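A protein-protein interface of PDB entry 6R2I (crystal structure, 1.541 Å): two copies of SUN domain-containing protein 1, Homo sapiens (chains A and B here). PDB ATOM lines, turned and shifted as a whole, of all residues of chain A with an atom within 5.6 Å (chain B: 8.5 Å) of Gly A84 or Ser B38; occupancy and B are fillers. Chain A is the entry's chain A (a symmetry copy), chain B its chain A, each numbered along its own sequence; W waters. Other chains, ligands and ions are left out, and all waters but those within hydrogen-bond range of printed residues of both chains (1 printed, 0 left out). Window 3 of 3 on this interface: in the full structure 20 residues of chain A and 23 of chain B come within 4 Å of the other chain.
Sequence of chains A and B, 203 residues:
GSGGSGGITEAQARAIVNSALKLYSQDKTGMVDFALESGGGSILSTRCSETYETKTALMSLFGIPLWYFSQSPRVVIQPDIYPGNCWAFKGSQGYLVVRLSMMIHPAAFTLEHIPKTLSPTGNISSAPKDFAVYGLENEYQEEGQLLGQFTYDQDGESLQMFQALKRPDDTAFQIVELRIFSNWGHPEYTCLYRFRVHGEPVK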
ATOM      1  N   GLN A  71      -2.259  14.910 -25.738  1.00  0.00           N
ATOM      2  CA  GLN A  71      -2.266  13.616 -25.075  1.00  0.00           C
ATOM      3  C   GLN A  71      -3.636  13.302 -24.486  1.00  0.00           C
ATOM      4  O   GLN A  71      -4.310  14.178 -23.935  1.00  0.00           O
ATOM      5  CB  GLN A  71      -1.233  13.598 -23.952  1.00  0.00           C
ATOM      6  CG  GLN A  71       0.178  13.971 -24.359  1.00  0.00           C
ATOM      7  CD  GLN A  71       0.953  12.845 -24.987  1.00  0.00           C
ATOM      8  OE1 GLN A  71       0.419  11.776 -25.271  1.00  0.00           O
ATOM      9  NE2 GLN A  71       2.251  13.077 -25.203  1.00  0.00           N
ATOM     10  N   TYR A  82       8.762  10.369 -19.842  1.00  0.00           N
ATOM     11  CA  TYR A  82       9.556  11.488 -20.356  1.00  0.00           C
ATOM     12  C   TYR A  82       8.721  12.779 -20.292  1.00  0.00           C
ATOM     13  O   TYR A  82       7.487  12.730 -20.407  1.00  0.00           O
ATOM     14  CB  TYR A  82      10.038  11.197 -21.815  1.00  0.00           C
ATOM     15  CG  TYR A  82      11.324  10.378 -21.803  1.00  0.00           C
ATOM     16  CD1 TYR A  82      11.305   9.017 -21.558  1.00  0.00           C
ATOM     17  CD2 TYR A  82      12.569  10.981 -21.983  1.00  0.00           C
ATOM     18  CE1 TYR A  82      12.485   8.272 -21.480  1.00  0.00           C
ATOM     19  CE2 TYR A  82      13.766  10.240 -21.887  1.00  0.00           C
ATOM     20  CZ  TYR A  82      13.707   8.886 -21.630  1.00  0.00           C
ATOM     21  OH  TYR A  82      14.891   8.148 -21.496  1.00  0.00           O
ATOM     22  N   PRO A  83       9.351  13.944 -20.132  1.00  0.00           N
ATOM     23  CA  PRO A  83       8.590  15.209 -20.117  1.00  0.00           C
ATOM     24  C   PRO A  83       7.606  15.336 -21.273  1.00  0.00           C
ATOM     25  O   PRO A  83       7.951  15.100 -22.440  1.00  0.00           O
ATOM     26  CB  PRO A  83       9.693  16.283 -20.198  1.00  0.00           C
ATOM     27  CG  PRO A  83      10.873  15.627 -19.473  1.00  0.00           C
ATOM     28  CD  PRO A  83      10.801  14.167 -19.909  1.00  0.00           C
ATOM     29  N   GLY A  84       6.355  15.706 -20.932  1.00  0.00           N
ATOM     30  CA  GLY A  84       5.269  15.823 -21.907  1.00  0.00           C
ATOM     31  C   GLY A  84       4.410  14.589 -22.102  1.00  0.00           C
ATOM     32  O   GLY A  84       3.322  14.696 -22.718  1.00  0.00           O
ATOM     33  N   ASN A  85       4.844  13.418 -21.615  1.00  0.00           N
ATOM     34  CA  ASN A  85       4.061  12.186 -21.746  1.00  0.00           C
ATOM     35  C   ASN A  85       3.110  12.041 -20.551  1.00  0.00           C
ATOM     36  O   ASN A  85       3.175  11.096 -19.751  1.00  0.00           O
ATOM     37  CB  ASN A  85       5.001  11.004 -21.924  1.00  0.00           C
ATOM     38  CG  ASN A  85       5.661  11.039 -23.326  1.00  0.00           C
ATOM     39  OD1 ASN A  85       5.100  11.624 -24.280  1.00  0.00           O
ATOM     40  ND2 ASN A  85       6.794  10.413 -23.459  1.00  0.00           N
ATOM     41  N   CYS A  86       2.198  13.015 -20.484  1.00  0.00           N
ATOM     42  CA  CYS A  86       1.300  13.286 -19.365  1.00  0.00           C
ATOM     43  C   CYS A  86      -0.017  13.821 -19.916  1.00  0.00           C
ATOM     44  O   CYS A  86      -0.057  14.407 -21.013  1.00  0.00           O
ATOM     45  CB  CYS A  86       1.898  14.308 -18.373  1.00  0.00           C
ATOM     46  SG  CYS A  86       2.517  15.857 -19.136  1.00  0.00           S
ATOM     47  N   TYR A 193       1.308  12.200 -14.938  1.00  0.00           N
ATOM     48  CA  TYR A 193       2.220  11.320 -15.674  1.00  0.00           C
ATOM     49  C   TYR A 193       1.865   9.833 -15.570  1.00  0.00           C
ATOM     50  O   TYR A 193       1.767   9.162 -16.610  1.00  0.00           O
ATOM     51  CB  TYR A 193       3.682  11.582 -15.232  1.00  0.00           C
ATOM     52  CG  TYR A 193       4.312  12.783 -15.921  1.00  0.00           C
ATOM     53  CD1 TYR A 193       4.137  14.075 -15.422  1.00  0.00           C
ATOM     54  CD2 TYR A 193       5.032  12.630 -17.116  1.00  0.00           C
ATOM     55  CE1 TYR A 193       4.687  15.192 -16.075  1.00  0.00           C
ATOM     56  CE2 TYR A 193       5.568  13.731 -17.775  1.00  0.00           C
ATOM     57  CZ  TYR A 193       5.382  15.017 -17.253  1.00  0.00           C
ATOM     58  OH  TYR A 193       5.910  16.098 -17.934  1.00  0.00           O
ATOM     59  N   ASP B  33      16.889  18.284 -21.306  1.00  0.00           N
ATOM     60  CA  ASP B  33      17.179  18.242 -22.748  1.00  0.00           C
ATOM     61  C   ASP B  33      16.160  19.138 -23.472  1.00  0.00           C
ATOM     62  O   ASP B  33      14.990  18.749 -23.643  1.00  0.00           O
ATOM     63  CB  ASP B  33      17.107  16.827 -23.298  1.00  0.00           C
ATOM     64  CG  ASP B  33      17.327  16.767 -24.812  1.00  0.00           C
ATOM     65  OD1 ASP B  33      17.695  17.801 -25.417  1.00  0.00           O
ATOM     66  OD2 ASP B  33      17.088  15.669 -25.374  1.00  0.00           O
ATOM     67  N   PHE B  34      16.599  20.344 -23.881  1.00  0.00           N
ATOM     68  CA  PHE B  34      15.715  21.301 -24.552  1.00  0.00           C
ATOM     69  C   PHE B  34      15.441  20.944 -26.014  1.00  0.00           C
ATOM     70  O   PHE B  34      14.575  21.608 -26.645  1.00  0.00           O
ATOM     71  CB  PHE B  34      16.303  22.719 -24.446  1.00  0.00           C
ATOM     72  CG  PHE B  34      16.324  23.271 -23.014  1.00  0.00           C
ATOM     73  CD1 PHE B  34      15.164  23.814 -22.450  1.00  0.00           C
ATOM     74  CD2 PHE B  34      17.471  23.215 -22.255  1.00  0.00           C
ATOM     75  CE1 PHE B  34      15.148  24.273 -21.163  1.00  0.00           C
ATOM     76  CE2 PHE B  34      17.490  23.683 -20.931  1.00  0.00           C
ATOM     77  CZ  PHE B  34      16.339  24.228 -20.382  1.00  0.00           C
ATOM     78  N   ALA B  35      16.087  19.892 -26.554  1.00  0.00           N
ATOM     79  CA  ALA B  35      15.756  19.388 -27.897  1.00  0.00           C
ATOM     80  C   ALA B  35      14.698  18.286 -27.907  1.00  0.00           C
ATOM     81  O   ALA B  35      14.107  18.036 -28.966  1.00  0.00           O
ATOM     82  CB  ALA B  35      17.025  18.865 -28.601  1.00  0.00           C
ATOM     83  N   LEU B  36      14.414  17.657 -26.771  1.00  0.00           N
ATOM     84  CA  LEU B  36      13.544  16.476 -26.719  1.00  0.00           C
ATOM     85  C   LEU B  36      12.162  16.803 -27.282  1.00  0.00           C
ATOM     86  O   LEU B  36      11.505  17.737 -26.836  1.00  0.00           O
ATOM     87  CB  LEU B  36      13.430  16.018 -25.254  1.00  0.00           C
ATOM     88  CG  LEU B  36      12.601  14.763 -24.964  1.00  0.00           C
ATOM     89  CD1 LEU B  36      13.348  13.527 -25.437  1.00  0.00           C
ATOM     90  CD2 LEU B  36      12.226  14.661 -23.472  1.00  0.00           C
ATOM     91  N   GLU B  37      11.687  15.973 -28.224  1.00  0.00           N
ATOM     92  CA  GLU B  37      10.434  16.299 -28.920  1.00  0.00           C
ATOM     93  C   GLU B  37       9.232  16.308 -27.976  1.00  0.00           C
ATOM     94  O   GLU B  37       8.400  17.239 -28.021  1.00  0.00           O
ATOM     95  CB  GLU B  37      10.194  15.312 -30.067  1.00  0.00           C
ATOM     96  CG  GLU B  37       9.060  15.757 -31.008  1.00  0.00           C
ATOM     97  CD  GLU B  37       8.834  14.799 -32.167  1.00  0.00           C
ATOM     98  OE1 GLU B  37       8.446  13.629 -31.897  1.00  0.00           O
ATOM     99  OE2 GLU B  37       9.048  15.209 -33.350  1.00  0.00           O
ATOM    100  N   SER B  38       9.112  15.305 -27.090  1.00  0.00           N
ATOM    101  CA  SER B  38       7.912  15.247 -26.250  1.00  0.00           C
ATOM    102  C   SER B  38       7.802  16.455 -25.307  1.00  0.00           C
ATOM    103  O   SER B  38       6.680  16.845 -24.922  1.00  0.00           O
ATOM    104  CB  SER B  38       7.897  13.938 -25.458  1.00  0.00           C
ATOM    105  OG  SER B  38       9.001  13.844 -24.559  1.00  0.00           O
ATOM    106  N   GLY B  39       8.925  17.069 -24.938  1.00  0.00           N
ATOM    107  CA  GLY B  39       8.915  18.242 -24.091  1.00  0.00           C
ATOM    108  C   GLY B  39       8.801  19.578 -24.793  1.00  0.00           C
ATOM    109  O   GLY B  39       8.774  20.625 -24.112  1.00  0.00           O
ATOM    110  N   GLY B  40       8.761  19.587 -26.133  1.00  0.00           N
ATOM    111  CA  GLY B  40       8.571  20.826 -26.889  1.00  0.00           C
ATOM    112  C   GLY B  40       9.600  21.152 -27.969  1.00  0.00           C
ATOM    113  O   GLY B  40       9.454  22.161 -28.686  1.00  0.00           O
ATOM    114  N   GLY B  41      10.611  20.290 -28.134  1.00  0.00           N
ATOM    115  CA  GLY B  41      11.536  20.424 -29.267  1.00  0.00           C
ATOM    116  C   GLY B  41      10.905  19.930 -30.575  1.00  0.00           C
ATOM    117  O   GLY B  41       9.971  19.134 -30.563  1.00  0.00           O
ATOM    118  N   SER B  42      11.444  20.384 -31.712  1.00  0.00           N
ATOM    119  CA  SER B  42      10.932  19.918 -33.005  1.00  0.00           C
ATOM    120  C   SER B  42      11.986  20.048 -34.090  1.00  0.00           C
ATOM    121  O   SER B  42      12.898  20.878 -34.004  1.00  0.00           O
ATOM    122  CB  SER B  42       9.668  20.672 -33.415  1.00  0.00           C
ATOM    123  OG  SER B  42       9.896  22.079 -33.515  1.00  0.00           O
ATOM    124  N   ARG B  74      13.030  12.992 -36.979  1.00  0.00           N
ATOM    125  CA  ARG B  74      12.393  13.089 -35.666  1.00  0.00           C
ATOM    126  C   ARG B  74      12.956  12.082 -34.667  1.00  0.00           C
ATOM    127  O   ARG B  74      12.957  12.358 -33.463  1.00  0.00           O
ATOM    128  CB  ARG B  74      10.872  12.903 -35.784  1.00  0.00           C
ATOM    129  CG  ARG B  74      10.121  14.040 -36.507  1.00  0.00           C
ATOM    130  CD  ARG B  74       8.634  13.722 -36.702  1.00  0.00           C
ATOM    131  NE  ARG B  74       7.998  13.521 -35.410  1.00  0.00           N
ATOM    132  CZ  ARG B  74       6.862  12.871 -35.179  1.00  0.00           C
ATOM    133  NH1 ARG B  74       6.128  12.338 -36.165  1.00  0.00           N
ATOM    134  NH2 ARG B  74       6.464  12.750 -33.918  1.00  0.00           N
ATOM    135  N   ILE B  77      15.488  13.096 -31.833  1.00  0.00           N
ATOM    136  CA  ILE B  77      15.053  13.774 -30.610  1.00  0.00           C
ATOM    137  C   ILE B  77      13.990  12.946 -29.876  1.00  0.00           C
ATOM    138  O   ILE B  77      13.128  13.490 -29.155  1.00  0.00           O
ATOM    139  CB  ILE B  77      14.610  15.229 -30.909  1.00  0.00           C
ATOM    140  CG1 ILE B  77      13.567  15.329 -32.010  1.00  0.00           C
ATOM    141  CG2 ILE B  77      15.845  16.067 -31.363  1.00  0.00           C
ATOM    142  CD1 ILE B  77      12.914  16.706 -32.101  1.00  0.00           C
ATOM    143  N   GLN B  78      14.118  11.612 -29.982  1.00  0.00           N
ATOM    144  CA  GLN B  78      13.351  10.599 -29.247  1.00  0.00           C
ATOM    145  C   GLN B  78      14.289   9.623 -28.536  1.00  0.00           C
ATOM    146  O   GLN B  78      15.369   9.292 -29.063  1.00  0.00           O
ATOM    147  CB  GLN B  78      12.387   9.866 -30.229  1.00  0.00           C
ATOM    148  CG  GLN B  78      11.400  10.807 -30.922  1.00  0.00           C
ATOM    149  CD  GLN B  78      10.581  10.151 -32.036  1.00  0.00           C
ATOM    150  OE1 GLN B  78      10.841   9.003 -32.422  1.00  0.00           O
ATOM    151  NE2 GLN B  78       9.597  10.888 -32.571  1.00  0.00           N
ATOM    152  N   PRO B  79      13.929   9.160 -27.329  1.00  0.00           N
ATOM    153  CA  PRO B  79      14.925   8.498 -26.462  1.00  0.00           C
ATOM    154  C   PRO B  79      15.303   7.040 -26.764  1.00  0.00           C
ATOM    155  O   PRO B  79      16.375   6.607 -26.314  1.00  0.00           O
ATOM    156  CB  PRO B  79      14.285   8.604 -25.060  1.00  0.00           C
ATOM    157  CG  PRO B  79      12.807   8.675 -25.312  1.00  0.00           C
ATOM    158  CD  PRO B  79      12.708   9.517 -26.574  1.00  0.00           C
ATOM    159  N   SER B 101      12.701  23.808 -26.946  1.00  0.00           N
ATOM    160  CA  SER B 101      11.482  24.046 -26.167  1.00  0.00           C
ATOM    161  C   SER B 101      11.502  25.360 -25.385  1.00  0.00           C
ATOM    162  O   SER B 101      10.434  25.804 -24.924  1.00  0.00           O
ATOM    163  CB  SER B 101      11.223  22.870 -25.213  1.00  0.00           C
ATOM    164  OG  SER B 101      12.304  22.710 -24.315  1.00  0.00           O
ATOM    165  N   ARG B 194      20.757   9.827 -31.124  1.00  0.00           N
ATOM    166  CA  ARG B 194      20.123  10.871 -30.323  1.00  0.00           C
ATOM    167  C   ARG B 194      21.082  12.036 -30.086  1.00  0.00           C
ATOM    168  O   ARG B 194      22.277  11.833 -29.805  1.00  0.00           O
ATOM    169  CB  ARG B 194      19.599  10.348 -28.966  1.00  0.00           C
ATOM    170  CG  ARG B 194      18.846  11.446 -28.193  1.00  0.00           C
ATOM    171  CD  ARG B 194      18.035  10.931 -27.008  1.00  0.00           C
ATOM    172  NE  ARG B 194      17.495  12.027 -26.215  1.00  0.00           N
ATOM    173  CZ  ARG B 194      17.226  11.948 -24.911  1.00  0.00           C
ATOM    174  NH1 ARG B 194      17.361  10.791 -24.267  1.00  0.00           N
ATOM    175  NH2 ARG B 194      16.833  13.024 -24.244  1.00  0.00           N
HETATM  176  O   HOH W   1       4.125  16.019 -25.776  1.00  0.00           O
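The side-chain hydroxyl of Ser B38 sits at hydrogen-bond distance from the backbone carbonyl oxygen of Pro A83.
The backbone carbonyl oxygen of Pro A83 is in hydrogen-bond range of the backbone NH of Gly B39, at 3.3 Å.
The backbone carbonyl oxygen of Leu B36 is in hydrogen-bond range of the backbone NH of Gly B41 (3.0 Å).
NE2 of Gln A71 sits at hydrogen-bond distance from O of Gly A84 (3.2 Å).
NE2 of Gln A71 lies within hydrogen-bond range of OD1 of Asn A85 (3.3 Å).
N of Gly A84 is in hydrogen-bond range of OH of Tyr A193 (3.1 Å).
Among the printed residues, merely in contact across the chains: Tyr A82 with Leu B36 (3.98 Å), Tyr A82 with Ser B38 (3.95 Å), Tyr A82 with Pro B79 (3.5 Å), Pro A83 with Leu B36 (3.9 Å), Gly A84 with Ser B38 (3.5 Å) and Asn A85 with Ser B38 (3.8 Å).
Of chain B, only Ser B38 (3.5 Å) comes within 4 Å of Gly A84.
Of chain A, only Tyr A82, Pro A83, Gly A84 and Asn A85 come within 4 Å of Ser B38.
Of chain B, only Ser B38 comes within 4 Å of Asn A85.
Printed residues of chain A within 4 Å of Gly B39: Pro A83 (3.3 Å).
Of the printed residues of chain B, Pro A83 touches Leu B36 (3.9 Å), Ser B38 (2.7 Å) and Gly B39 (3.3 Å).
Of the printed residues of chain A, Pro B79 touches Tyr A82 (3.5 Å).
Printed residues of chain A within 4 Å of Leu B36: Tyr A82 and Pro A83.
Of the printed residues of chain B, Tyr A82 touches Leu B36, Ser B38 and Pro B79.
The nearest residue of chain B that does not touch Gly A84 is Gly B39 (4.8 Å).
The nearest printed residue of chain A that does not touch Ser B38 is Gln A71 (5.7 Å).
The nearest printed residue of chain B that does not touch Tyr A82 is Arg B194 (4.3 Å).
Printed residues of chain A that touch a printed residue of chain B: Tyr A82, Pro A83, Gly A84 and Asn A85.
Hydrophobic or aromatic side chains of chain B within 4 Å of the printed part of chain A: Leu B36 and Pro B79.
Among the printed residues, 8 pairs touch across the chains.
Among the printed residues, no Asp or Glu carboxylate lies within 4 Å of a Lys or Arg side-chain nitrogen of the other chain.
No position is printed for both chains.
Of the 8 pairs that touch across the chains among the printed residues, none has its exchanged pair printed and touching as well.
Water W1 lies within hydrogen-bond range of the backbone carbonyl oxygen (O) of Ser B38 (2.8 Å) and the backbone carbonyl oxygen (O) of Gly A84 (3.4 Å).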
